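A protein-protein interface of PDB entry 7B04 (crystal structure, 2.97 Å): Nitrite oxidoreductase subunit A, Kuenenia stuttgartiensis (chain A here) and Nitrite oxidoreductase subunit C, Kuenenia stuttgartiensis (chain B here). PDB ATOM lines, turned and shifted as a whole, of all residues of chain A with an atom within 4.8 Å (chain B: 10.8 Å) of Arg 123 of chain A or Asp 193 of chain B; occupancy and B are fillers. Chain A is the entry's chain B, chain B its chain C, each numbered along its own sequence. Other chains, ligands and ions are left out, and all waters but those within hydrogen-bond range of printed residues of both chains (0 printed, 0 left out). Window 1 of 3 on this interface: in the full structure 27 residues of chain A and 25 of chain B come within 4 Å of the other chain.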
ATOM      1  N   THR A 120       4.425   0.538 -27.604  1.00  0.00           N
ATOM      2  CA  THR A 120       3.052   0.991 -27.805  1.00  0.00           C
ATOM      3  C   THR A 120       2.417   0.397 -29.054  1.00  0.00           C
ATOM      4  O   THR A 120       1.446   0.957 -29.577  1.00  0.00           O
ATOM      5  CB  THR A 120       2.989   2.523 -27.846  1.00  0.00           C
ATOM      6  OG1 THR A 120       3.401   2.989 -29.135  1.00  0.00           O
ATOM      7  CG2 THR A 120       3.876   3.124 -26.778  1.00  0.00           C
ATOM      8  N   PHE A 121       2.952  -0.716 -29.560  1.00  0.00           N
ATOM      9  CA  PHE A 121       2.388  -1.317 -30.770  1.00  0.00           C
ATOM     10  C   PHE A 121       0.981  -1.849 -30.535  1.00  0.00           C
ATOM     11  O   PHE A 121       0.142  -1.830 -31.444  1.00  0.00           O
ATOM     12  CB  PHE A 121       3.280  -2.443 -31.275  1.00  0.00           C
ATOM     13  CG  PHE A 121       2.751  -3.103 -32.508  1.00  0.00           C
ATOM     14  CD1 PHE A 121       2.399  -2.342 -33.613  1.00  0.00           C
ATOM     15  CD2 PHE A 121       2.566  -4.467 -32.552  1.00  0.00           C
ATOM     16  CE1 PHE A 121       1.900  -2.945 -34.745  1.00  0.00           C
ATOM     17  CE2 PHE A 121       2.067  -5.073 -33.681  1.00  0.00           C
ATOM     18  CZ  PHE A 121       1.733  -4.312 -34.777  1.00  0.00           C
ATOM     19  N   HIS A 122       0.700  -2.337 -29.329  1.00  0.00           N
ATOM     20  CA  HIS A 122      -0.634  -2.856 -29.019  1.00  0.00           C
ATOM     21  C   HIS A 122      -1.676  -1.756 -28.999  1.00  0.00           C
ATOM     22  O   HIS A 122      -2.864  -2.032 -29.203  1.00  0.00           O
ATOM     23  CB  HIS A 122      -0.621  -3.614 -27.697  1.00  0.00           C
ATOM     24  CG  HIS A 122      -0.207  -2.779 -26.516  1.00  0.00           C
ATOM     25  ND1 HIS A 122       1.082  -2.304 -26.350  1.00  0.00           N
ATOM     26  CD2 HIS A 122      -0.909  -2.358 -25.436  1.00  0.00           C
ATOM     27  CE1 HIS A 122       1.151  -1.627 -25.222  1.00  0.00           C
ATOM     28  NE2 HIS A 122      -0.040  -1.646 -24.651  1.00  0.00           N
ATOM     29  N   ARG A 123      -1.265  -0.523 -28.715  1.00  0.00           N
ATOM     30  CA  ARG A 123      -2.194   0.597 -28.840  1.00  0.00           C
ATOM     31  C   ARG A 123      -2.662   0.775 -30.275  1.00  0.00           C
ATOM     32  O   ARG A 123      -3.765   1.275 -30.522  1.00  0.00           O
ATOM     33  CB  ARG A 123      -1.528   1.881 -28.339  1.00  0.00           C
ATOM     34  CG  ARG A 123      -2.053   2.334 -27.013  1.00  0.00           C
ATOM     35  CD  ARG A 123      -3.389   3.012 -27.194  1.00  0.00           C
ATOM     36  NE  ARG A 123      -4.165   3.054 -25.965  1.00  0.00           N
ATOM     37  CZ  ARG A 123      -4.360   4.164 -25.270  1.00  0.00           C
ATOM     38  NH1 ARG A 123      -5.031   4.132 -24.129  1.00  0.00           N
ATOM     39  NH2 ARG A 123      -3.819   5.298 -25.687  1.00  0.00           N
ATOM     40  N   ARG A 124      -1.841   0.359 -31.226  1.00  0.00           N
ATOM     41  CA  ARG A 124      -2.241   0.376 -32.625  1.00  0.00           C
ATOM     42  C   ARG A 124      -3.023  -0.880 -32.971  1.00  0.00           C
ATOM     43  O   ARG A 124      -3.903  -0.860 -33.839  1.00  0.00           O
ATOM     44  CB  ARG A 124      -1.010   0.479 -33.526  1.00  0.00           C
ATOM     45  CG  ARG A 124      -0.211   1.738 -33.396  1.00  0.00           C
ATOM     46  CD  ARG A 124       1.045   1.590 -34.228  1.00  0.00           C
ATOM     47  NE  ARG A 124       0.703   1.518 -35.647  1.00  0.00           N
ATOM     48  CZ  ARG A 124       1.535   1.106 -36.599  1.00  0.00           C
ATOM     49  NH1 ARG A 124       1.138   1.061 -37.868  1.00  0.00           N
ATOM     50  NH2 ARG A 124       2.767   0.721 -36.283  1.00  0.00           N
ATOM     51  N   VAL A 125      -2.693  -1.987 -32.309  1.00  0.00           N
ATOM     52  CA  VAL A 125      -3.341  -3.263 -32.591  1.00  0.00           C
ATOM     53  C   VAL A 125      -4.824  -3.200 -32.228  1.00  0.00           C
ATOM     54  O   VAL A 125      -5.695  -3.602 -33.009  1.00  0.00           O
ATOM     55  CB  VAL A 125      -2.617  -4.383 -31.823  1.00  0.00           C
ATOM     56  CG1 VAL A 125      -3.386  -5.678 -31.951  1.00  0.00           C
ATOM     57  CG2 VAL A 125      -1.191  -4.541 -32.323  1.00  0.00           C
ATOM     58  N   TYR A 126      -5.137  -2.665 -31.049  1.00  0.00           N
ATOM     59  CA  TYR A 126      -6.523  -2.470 -30.629  1.00  0.00           C
ATOM     60  C   TYR A 126      -6.955  -1.016 -30.771  1.00  0.00           C
ATOM     61  O   TYR A 126      -7.680  -0.490 -29.923  1.00  0.00           O
ATOM     62  CB  TYR A 126      -6.727  -2.946 -29.197  1.00  0.00           C
ATOM     63  CG  TYR A 126      -6.263  -4.353 -28.907  1.00  0.00           C
ATOM     64  CD1 TYR A 126      -7.050  -5.449 -29.240  1.00  0.00           C
ATOM     65  CD2 TYR A 126      -5.044  -4.587 -28.286  1.00  0.00           C
ATOM     66  CE1 TYR A 126      -6.630  -6.741 -28.964  1.00  0.00           C
ATOM     67  CE2 TYR A 126      -4.617  -5.873 -28.007  1.00  0.00           C
ATOM     68  CZ  TYR A 126      -5.414  -6.946 -28.348  1.00  0.00           C
ATOM     69  OH  TYR A 126      -4.986  -8.223 -28.069  1.00  0.00           O
ATOM     70  N   GLY A 127      -6.554  -0.347 -31.849  1.00  0.00           N
ATOM     71  CA  GLY A 127      -6.749   1.078 -31.958  1.00  0.00           C
ATOM     72  C   GLY A 127      -7.884   1.486 -32.872  1.00  0.00           C
ATOM     73  O   GLY A 127      -8.495   0.664 -33.567  1.00  0.00           O
ATOM     74  N   THR A 929      -0.634   7.364 -33.369  1.00  0.00           N
ATOM     75  CA  THR A 929      -0.942   6.700 -32.111  1.00  0.00           C
ATOM     76  C   THR A 929      -0.857   7.689 -30.961  1.00  0.00           C
ATOM     77  O   THR A 929       0.183   8.322 -30.764  1.00  0.00           O
ATOM     78  CB  THR A 929       0.029   5.547 -31.897  1.00  0.00           C
ATOM     79  OG1 THR A 929       0.027   4.724 -33.066  1.00  0.00           O
ATOM     80  CG2 THR A 929      -0.380   4.721 -30.687  1.00  0.00           C
ATOM     81  N   ASP A 930      -1.939   7.790 -30.184  1.00  0.00           N
ATOM     82  CA  ASP A 930      -2.090   8.889 -29.233  1.00  0.00           C
ATOM     83  C   ASP A 930      -0.857   9.059 -28.349  1.00  0.00           C
ATOM     84  O   ASP A 930      -0.330  10.169 -28.215  1.00  0.00           O
ATOM     85  CB  ASP A 930      -3.342   8.677 -28.384  1.00  0.00           C
ATOM     86  CG  ASP A 930      -3.340   7.351 -27.668  1.00  0.00           C
ATOM     87  OD1 ASP A 930      -2.395   6.556 -27.868  1.00  0.00           O
ATOM     88  OD2 ASP A 930      -4.291   7.096 -26.902  1.00  0.00           O
ATOM     89  N   TRP A 931      -0.375   7.969 -27.747  1.00  0.00           N
ATOM     90  CA  TRP A 931       0.747   8.069 -26.817  1.00  0.00           C
ATOM     91  C   TRP A 931       1.981   8.656 -27.494  1.00  0.00           C
ATOM     92  O   TRP A 931       2.598   9.595 -26.978  1.00  0.00           O
ATOM     93  CB  TRP A 931       1.056   6.695 -26.222  1.00  0.00           C
ATOM     94  CG  TRP A 931       0.055   6.252 -25.199  1.00  0.00           C
ATOM     95  CD1 TRP A 931      -0.898   7.020 -24.598  1.00  0.00           C
ATOM     96  CD2 TRP A 931      -0.094   4.932 -24.660  1.00  0.00           C
ATOM     97  NE1 TRP A 931      -1.631   6.262 -23.716  1.00  0.00           N
ATOM     98  CE2 TRP A 931      -1.157   4.976 -23.737  1.00  0.00           C
ATOM     99  CE3 TRP A 931       0.567   3.719 -24.869  1.00  0.00           C
ATOM    100  CZ2 TRP A 931      -1.572   3.855 -23.023  1.00  0.00           C
ATOM    101  CZ3 TRP A 931       0.154   2.607 -24.158  1.00  0.00           C
ATOM    102  CH2 TRP A 931      -0.905   2.682 -23.248  1.00  0.00           C
ATOM    103  N   GLU B 183     -17.421  11.194 -15.284  1.00  0.00           N
ATOM    104  CA  GLU B 183     -16.119  10.766 -15.772  1.00  0.00           C
ATOM    105  C   GLU B 183     -15.484  11.881 -16.601  1.00  0.00           C
ATOM    106  O   GLU B 183     -16.094  12.922 -16.858  1.00  0.00           O
ATOM    107  CB  GLU B 183     -16.242   9.447 -16.538  1.00  0.00           C
ATOM    108  CG  GLU B 183     -16.998   8.385 -15.741  1.00  0.00           C
ATOM    109  CD  GLU B 183     -16.678   6.966 -16.171  1.00  0.00           C
ATOM    110  OE1 GLU B 183     -15.857   6.791 -17.096  1.00  0.00           O
ATOM    111  OE2 GLU B 183     -17.247   6.025 -15.578  1.00  0.00           O
ATOM    112  N   CYS B 184     -14.239  11.645 -17.018  1.00  0.00           N
ATOM    113  CA  CYS B 184     -13.416  12.713 -17.585  1.00  0.00           C
ATOM    114  C   CYS B 184     -14.032  13.469 -18.763  1.00  0.00           C
ATOM    115  O   CYS B 184     -13.878  14.702 -18.800  1.00  0.00           O
ATOM    116  CB  CYS B 184     -12.050  12.137 -17.980  1.00  0.00           C
ATOM    117  SG  CYS B 184     -11.096  11.536 -16.574  1.00  0.00           S
ATOM    118  N   PRO B 185     -14.699  12.839 -19.739  1.00  0.00           N
ATOM    119  CA  PRO B 185     -15.256  13.631 -20.852  1.00  0.00           C
ATOM    120  C   PRO B 185     -16.220  14.723 -20.415  1.00  0.00           C
ATOM    121  O   PRO B 185     -16.428  15.680 -21.173  1.00  0.00           O
ATOM    122  CB  PRO B 185     -15.958  12.577 -21.718  1.00  0.00           C
ATOM    123  CG  PRO B 185     -15.211  11.330 -21.446  1.00  0.00           C
ATOM    124  CD  PRO B 185     -14.842  11.394 -19.991  1.00  0.00           C
ATOM    125  N   TYR B 188     -13.477  17.404 -19.918  1.00  0.00           N
ATOM    126  CA  TYR B 188     -12.687  17.665 -21.121  1.00  0.00           C
ATOM    127  C   TYR B 188     -13.415  17.053 -22.312  1.00  0.00           C
ATOM    128  O   TYR B 188     -13.080  15.947 -22.759  1.00  0.00           O
ATOM    129  CB  TYR B 188     -11.270  17.110 -20.979  1.00  0.00           C
ATOM    130  CG  TYR B 188     -10.524  17.658 -19.784  1.00  0.00           C
ATOM    131  CD1 TYR B 188     -10.004  18.946 -19.798  1.00  0.00           C
ATOM    132  CD2 TYR B 188     -10.340  16.891 -18.640  1.00  0.00           C
ATOM    133  CE1 TYR B 188      -9.322  19.454 -18.708  1.00  0.00           C
ATOM    134  CE2 TYR B 188      -9.656  17.389 -17.546  1.00  0.00           C
ATOM    135  CZ  TYR B 188      -9.150  18.673 -17.586  1.00  0.00           C
ATOM    136  OH  TYR B 188      -8.471  19.178 -16.501  1.00  0.00           O
ATOM    137  N   PRO B 189     -14.421  17.746 -22.852  1.00  0.00           N
ATOM    138  CA  PRO B 189     -15.252  17.138 -23.905  1.00  0.00           C
ATOM    139  C   PRO B 189     -14.523  16.895 -25.216  1.00  0.00           C
ATOM    140  O   PRO B 189     -15.039  16.144 -26.055  1.00  0.00           O
ATOM    141  CB  PRO B 189     -16.390  18.152 -24.081  1.00  0.00           C
ATOM    142  CG  PRO B 189     -15.792  19.452 -23.658  1.00  0.00           C
ATOM    143  CD  PRO B 189     -14.830  19.130 -22.549  1.00  0.00           C
ATOM    144  N   ASN B 190     -13.352  17.490 -25.426  1.00  0.00           N
ATOM    145  CA  ASN B 190     -12.599  17.302 -26.660  1.00  0.00           C
ATOM    146  C   ASN B 190     -11.606  16.149 -26.583  1.00  0.00           C
ATOM    147  O   ASN B 190     -10.893  15.899 -27.562  1.00  0.00           O
ATOM    148  CB  ASN B 190     -11.851  18.589 -27.023  1.00  0.00           C
ATOM    149  CG  ASN B 190     -12.780  19.762 -27.251  1.00  0.00           C
ATOM    150  OD1 ASN B 190     -13.871  19.610 -27.798  1.00  0.00           O
ATOM    151  ND2 ASN B 190     -12.348  20.945 -26.832  1.00  0.00           N
ATOM    152  N   MET B 191     -11.544  15.448 -25.455  1.00  0.00           N
ATOM    153  CA  MET B 191     -10.534  14.422 -25.244  1.00  0.00           C
ATOM    154  C   MET B 191     -10.720  13.247 -26.200  1.00  0.00           C
ATOM    155  O   MET B 191     -11.814  12.983 -26.708  1.00  0.00           O
ATOM    156  CB  MET B 191     -10.568  13.922 -23.799  1.00  0.00           C
ATOM    157  CG  MET B 191     -11.784  13.086 -23.444  1.00  0.00           C
ATOM    158  SD  MET B 191     -11.696  12.465 -21.752  1.00  0.00           S
ATOM    159  CE  MET B 191     -10.386  11.253 -21.902  1.00  0.00           C
ATOM    160  N   HIS B 192      -9.619  12.540 -26.445  1.00  0.00           N
ATOM    161  CA  HIS B 192      -9.640  11.304 -27.213  1.00  0.00           C
ATOM    162  C   HIS B 192      -8.622  10.337 -26.630  1.00  0.00           C
ATOM    163  O   HIS B 192      -7.479  10.717 -26.357  1.00  0.00           O
ATOM    164  CB  HIS B 192      -9.337  11.545 -28.696  1.00  0.00           C
ATOM    165  CG  HIS B 192      -9.175  10.281 -29.482  1.00  0.00           C
ATOM    166  ND1 HIS B 192     -10.238   9.461 -29.796  1.00  0.00           N
ATOM    167  CD2 HIS B 192      -8.074   9.685 -30.000  1.00  0.00           C
ATOM    168  CE1 HIS B 192      -9.801   8.420 -30.482  1.00  0.00           C
ATOM    169  NE2 HIS B 192      -8.492   8.532 -30.620  1.00  0.00           N
ATOM    170  N   ASP B 193      -9.047   9.091 -26.441  1.00  0.00           N
ATOM    171  CA  ASP B 193      -8.187   7.998 -26.011  1.00  0.00           C
ATOM    172  C   ASP B 193      -8.394   6.837 -26.972  1.00  0.00           C
ATOM    173  O   ASP B 193      -9.531   6.508 -27.322  1.00  0.00           O
ATOM    174  CB  ASP B 193      -8.523   7.589 -24.573  1.00  0.00           C
ATOM    175  CG  ASP B 193      -7.514   6.629 -23.981  1.00  0.00           C
ATOM    176  OD1 ASP B 193      -6.424   7.085 -23.577  1.00  0.00           O
ATOM    177  OD2 ASP B 193      -7.821   5.422 -23.908  1.00  0.00           O
ATOM    178  N   ASP B 194      -7.295   6.213 -27.396  1.00  0.00           N
ATOM    179  CA  ASP B 194      -7.394   5.172 -28.413  1.00  0.00           C
ATOM    180  C   ASP B 194      -8.068   3.896 -27.923  1.00  0.00           C
ATOM    181  O   ASP B 194      -8.440   3.060 -28.753  1.00  0.00           O
ATOM    182  CB  ASP B 194      -6.008   4.849 -28.971  1.00  0.00           C
ATOM    183  CG  ASP B 194      -5.483   5.937 -29.893  1.00  0.00           C
ATOM    184  OD1 ASP B 194      -6.303   6.730 -30.402  1.00  0.00           O
ATOM    185  OD2 ASP B 194      -4.256   5.987 -30.130  1.00  0.00           O
ATOM    186  N   PHE B 195      -8.242   3.722 -26.617  1.00  0.00           N
ATOM    187  CA  PHE B 195      -8.979   2.588 -26.082  1.00  0.00           C
ATOM    188  C   PHE B 195     -10.328   2.991 -25.507  1.00  0.00           C
ATOM    189  O   PHE B 195     -11.358   2.412 -25.868  1.00  0.00           O
ATOM    190  CB  PHE B 195      -8.153   1.868 -25.008  1.00  0.00           C
ATOM    191  CG  PHE B 195      -7.029   1.045 -25.555  1.00  0.00           C
ATOM    192  CD1 PHE B 195      -6.915   0.815 -26.918  1.00  0.00           C
ATOM    193  CD2 PHE B 195      -6.099   0.476 -24.705  1.00  0.00           C
ATOM    194  CE1 PHE B 195      -5.881   0.046 -27.421  1.00  0.00           C
ATOM    195  CE2 PHE B 195      -5.065  -0.296 -25.201  1.00  0.00           C
ATOM    196  CZ  PHE B 195      -4.956  -0.511 -26.561  1.00  0.00           C
ATOM    197  N   SER B 196     -10.351   3.970 -24.608  1.00  0.00           N
ATOM    198  CA  SER B 196     -11.596   4.323 -23.955  1.00  0.00           C
ATOM    199  C   SER B 196     -12.534   5.081 -24.882  1.00  0.00           C
ATOM    200  O   SER B 196     -13.747   5.054 -24.652  1.00  0.00           O
ATOM    201  CB  SER B 196     -11.332   5.135 -22.682  1.00  0.00           C
ATOM    202  OG  SER B 196     -10.845   6.435 -22.971  1.00  0.00           O
ATOM    203  N   THR B 197     -12.034   5.807 -25.873  1.00  0.00           N
ATOM    204  CA  THR B 197     -12.952   6.577 -26.754  1.00  0.00           C
ATOM    205  C   THR B 197     -13.048   5.935 -28.134  1.00  0.00           C
ATOM    206  O   THR B 197     -13.384   6.632 -29.042  1.00  0.00           O
ATOM    207  CB  THR B 197     -12.649   8.078 -26.792  1.00  0.00           C
ATOM    208  OG1 THR B 197     -11.257   8.324 -26.678  1.00  0.00           O
ATOM    209  CG2 THR B 197     -13.303   8.832 -25.667  1.00  0.00           C
ATOM    210  N   ASN B 198     -12.744   4.653 -28.247  1.00  0.00           N
ATOM    211  CA  ASN B 198     -12.769   3.895 -29.516  1.00  0.00           C
ATOM    212  C   ASN B 198     -14.148   3.284 -29.740  1.00  0.00           C
ATOM    213  O   ASN B 198     -14.556   2.466 -28.951  1.00  0.00           O
ATOM    214  CB  ASN B 198     -11.822   2.720 -29.370  1.00  0.00           C
ATOM    215  CG  ASN B 198     -11.581   1.931 -30.624  1.00  0.00           C
ATOM    216  OD1 ASN B 198     -12.398   1.869 -31.509  1.00  0.00           O
ATOM    217  ND2 ASN B 198     -10.450   1.294 -30.687  1.00  0.00           N
ATOM    218  N   PRO B 199     -14.901   3.679 -30.775  1.00  0.00           N
ATOM    219  CA  PRO B 199     -16.221   3.101 -31.057  1.00  0.00           C
ATOM    220  C   PRO B 199     -16.157   1.693 -31.611  1.00  0.00           C
ATOM    221  O   PRO B 199     -17.204   1.045 -31.723  1.00  0.00           O
ATOM    222  CB  PRO B 199     -16.816   4.072 -32.086  1.00  0.00           C
ATOM    223  CG  PRO B 199     -15.977   5.325 -31.980  1.00  0.00           C
ATOM    224  CD  PRO B 199     -14.612   4.834 -31.639  1.00  0.00           C
ATOM    225  N   HIS B 200     -14.967   1.190 -31.938  1.00  0.00           N
ATOM    226  CA  HIS B 200     -14.804  -0.124 -32.545  1.00  0.00           C
ATOM    227  C   HIS B 200     -14.166  -1.124 -31.599  1.00  0.00           C
ATOM    228  O   HIS B 200     -13.718  -2.180 -32.047  1.00  0.00           O
ATOM    229  CB  HIS B 200     -13.959  -0.025 -33.812  1.00  0.00           C
ATOM    230  CG  HIS B 200     -14.460   0.984 -34.793  1.00  0.00           C
ATOM    231  ND1 HIS B 200     -15.572   0.765 -35.575  1.00  0.00           N
ATOM    232  CD2 HIS B 200     -14.010   2.220 -35.112  1.00  0.00           C
ATOM    233  CE1 HIS B 200     -15.785   1.821 -36.338  1.00  0.00           C
ATOM    234  NE2 HIS B 200     -14.851   2.718 -36.078  1.00  0.00           N
ATOM    235  N   SER B 201     -14.120  -0.822 -30.308  1.00  0.00           N
ATOM    236  CA  SER B 201     -13.442  -1.692 -29.356  1.00  0.00           C
ATOM    237  C   SER B 201     -14.085  -3.068 -29.314  1.00  0.00           C
ATOM    238  O   SER B 201     -15.305  -3.195 -29.171  1.00  0.00           O
ATOM    239  CB  SER B 201     -13.453  -1.062 -27.963  1.00  0.00           C
ATOM    240  OG  SER B 201     -12.602   0.079 -27.920  1.00  0.00           O
ATOM    241  N   HIS B 205     -11.510  -6.992 -25.317  1.00  0.00           N
ATOM    242  CA  HIS B 205     -10.447  -6.031 -25.052  1.00  0.00           C
ATOM    243  C   HIS B 205     -10.896  -5.014 -24.017  1.00  0.00           C
ATOM    244  O   HIS B 205     -10.249  -4.835 -22.980  1.00  0.00           O
ATOM    245  CB  HIS B 205     -10.022  -5.322 -26.343  1.00  0.00           C
ATOM    246  CG  HIS B 205      -8.960  -4.275 -26.121  1.00  0.00           C
ATOM    247  ND1 HIS B 205      -9.229  -2.918 -26.165  1.00  0.00           N
ATOM    248  CD2 HIS B 205      -7.642  -4.397 -25.826  1.00  0.00           C
ATOM    249  CE1 HIS B 205      -8.118  -2.253 -25.924  1.00  0.00           C
ATOM    250  NE2 HIS B 205      -7.146  -3.125 -25.717  1.00  0.00           N
ATOM    251  N   LYS B 206     -12.020  -4.353 -24.276  1.00  0.00           N
ATOM    252  CA  LYS B 206     -12.566  -3.388 -23.326  1.00  0.00           C
ATOM    253  C   LYS B 206     -12.907  -4.043 -21.987  1.00  0.00           C
ATOM    254  O   LYS B 206     -12.767  -3.412 -20.930  1.00  0.00           O
ATOM    255  CB  LYS B 206     -13.811  -2.712 -23.919  1.00  0.00           C
ATOM    256  CG  LYS B 206     -14.214  -1.412 -23.242  1.00  0.00           C
ATOM    257  CD  LYS B 206     -15.294  -0.723 -24.080  1.00  0.00           C
ATOM    258  CE  LYS B 206     -15.353   0.772 -23.799  1.00  0.00           C
ATOM    259  NZ  LYS B 206     -15.240   1.557 -25.064  1.00  0.00           N
ATOM    260  N   ILE B 209      -9.499  -4.324 -20.195  1.00  0.00           N
ATOM    261  CA  ILE B 209      -8.836  -3.049 -19.933  1.00  0.00           C
ATOM    262  C   ILE B 209      -9.603  -2.240 -18.896  1.00  0.00           C
ATOM    263  O   ILE B 209      -9.009  -1.646 -17.988  1.00  0.00           O
ATOM    264  CB  ILE B 209      -8.658  -2.261 -21.244  1.00  0.00           C
ATOM    265  CG1 ILE B 209      -7.710  -3.003 -22.188  1.00  0.00           C
ATOM    266  CG2 ILE B 209      -8.139  -0.860 -20.959  1.00  0.00           C
ATOM    267  CD1 ILE B 209      -6.324  -3.212 -21.621  1.00  0.00           C
ATOM    268  N   GLN B 210     -10.931  -2.206 -19.002  1.00  0.00           N
ATOM    269  CA  GLN B 210     -11.760  -1.474 -18.055  1.00  0.00           C
ATOM    270  C   GLN B 210     -12.341  -2.374 -16.970  1.00  0.00           C
ATOM    271  O   GLN B 210     -13.359  -2.027 -16.364  1.00  0.00           O
ATOM    272  CB  GLN B 210     -12.870  -0.722 -18.791  1.00  0.00           C
ATOM    273  CG  GLN B 210     -12.341   0.372 -19.707  1.00  0.00           C
ATOM    274  CD  GLN B 210     -13.432   1.276 -20.242  1.00  0.00           C
ATOM    275  OE1 GLN B 210     -14.600   1.144 -19.877  1.00  0.00           O
ATOM    276  NE2 GLN B 210     -13.055   2.206 -21.114  1.00  0.00           N
ATOM    277  N   GLU B 214      -7.893  -3.719 -13.647  1.00  0.00           N
ATOM    278  CA  GLU B 214      -7.056  -2.911 -14.552  1.00  0.00           C
ATOM    279  C   GLU B 214      -7.386  -1.440 -14.407  1.00  0.00           C
ATOM    280  O   GLU B 214      -6.596  -0.634 -14.845  1.00  0.00           O
ATOM    281  CB  GLU B 214      -7.191  -3.430 -15.966  1.00  0.00           C
ATOM    282  CG  GLU B 214      -6.629  -4.808 -16.083  1.00  0.00           C
ATOM    283  CD  GLU B 214      -5.141  -4.791 -15.925  1.00  0.00           C
ATOM    284  OE1 GLU B 214      -4.539  -3.944 -16.475  1.00  0.00           O
ATOM    285  OE2 GLU B 214      -4.627  -5.608 -15.247  1.00  0.00           O
ATOM    286  N   LEU B 215      -8.528  -1.120 -13.826  1.00  0.00           N
ATOM    287  CA  LEU B 215      -8.795   0.317 -13.649  1.00  0.00           C
ATOM    288  C   LEU B 215      -7.815   0.846 -12.600  1.00  0.00           C
ATOM    289  O   LEU B 215      -7.231   1.888 -12.839  1.00  0.00           O
ATOM    290  CB  LEU B 215     -10.258   0.475 -13.250  1.00  0.00           C
ATOM    291  CG  LEU B 215     -11.236   0.567 -14.413  1.00  0.00           C
ATOM    292  CD1 LEU B 215     -12.657   0.403 -13.954  1.00  0.00           C
ATOM    293  CD2 LEU B 215     -11.082   1.878 -15.141  1.00  0.00           C
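The side-chain carboxylate (OD2) of Asp 193 of chain B lies within salt-bridge range of the guanidinium group (NH1) of Arg 123 of chain A (3.1 Å). The backbone carbonyl oxygen (O) of Tyr 126 of chain A sits at hydrogen-bond distance from the side-chain amide nitrogen (ND2) of Asn 198 of chain B, 3.4 Å away. OD2 of Asp 194 of chain B lies within hydrogen-bond range of N of Asp 930 of chain A, at 2.9 Å.
NH2 of Arg 123 of chain A is in salt-bridge range of OD1 of Asp 930 of chain A. OD2 of Asp 193 of chain B sits close to N of Phe 195 of chain B. OD2 of Asp 193 of chain B is in hydrogen-bond range of N of Ser 196 of chain B, 3.0 Å away. The side-chain amide nitrogen (ND2) of Asn 198 of chain B is in hydrogen-bond range of the backbone carbonyl oxygen (O) of Asp 194 of chain B, at 3.3 Å. N of His 200 of chain B lies within hydrogen-bond range of OD1 of Asn 198 of chain B (2.7 Å). The backbone carbonyl oxygen (O) of Asn 198 of chain B lies close to the side-chain hydroxyl (OG) of Ser 201 of chain B (3.3 Å).
Among the printed residues, merely in contact across the chains: His 122 of chain A with Phe 195 of chain B (3.7 Å), Arg 123 of chain A with Asp 194 of chain B (3.7 Å), Arg 123 of chain A with Phe 195 of chain B (3.5 Å), Tyr 126 of chain A with Asp 194 of chain B (3.8 Å), Tyr 126 of chain A with Phe 195 of chain B (3.1 Å), Tyr 126 of chain A with His 205 of chain B (3.4 Å), Gly 127 of chain A with Asn 198 of chain B (3.4 Å), Thr 929 of chain A with Asp 194 of chain B (3.9 Å) and Asp 930 of chain A with Asp 193 of chain B (3.95 Å).
No residue of chain B comes within 4 Å of Thr 120 of chain A. Of chain B, only Phe 195 comes within 4 Å of His 122 of chain A. Arg 123 of chain A touches just these residues of chain B: Asp 193 (3.1 Å), Asp 194 (3.7 Å) and Phe 195 (3.5 Å). No residue of chain B comes within 4 Å of Val 125 of chain A. Of chain B, only Asn 198 comes within 4 Å of Gly 127 of chain A. Printed residues of chain B within 4 Å of Thr 929 of chain A: Asp 194. Asp 930 of chain A touches just these residues of chain B: Asp 193 (3.95 Å) and Asp 194 (2.9 Å). Asp 193 of chain B touches just these residues of chain A: Arg 123 and Asp 930. Of the printed residues of chain A, Asp 194 of chain B touches Arg 123, Tyr 126, Thr 929 and Asp 930. Of the printed residues of chain A, Phe 195 of chain B touches His 122 (3.7 Å), Arg 123 (3.5 Å) and Tyr 126 (3.1 Å). The nearest residue of chain B that does not touch Arg 123 of chain A is Ser 196 of chain B (5.3 Å).
Of the 11 printed residues of chain A, 6 touch a printed residue of chain B. Among the printed residues, 12 pairs touch across the chains. Among the printed residues, Asp or Glu carboxylates within 4 Å of a Lys or Arg side-chain nitrogen of the other chain: Arg 123 of chain A with Asp 193 of chain B (3.1 Å).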
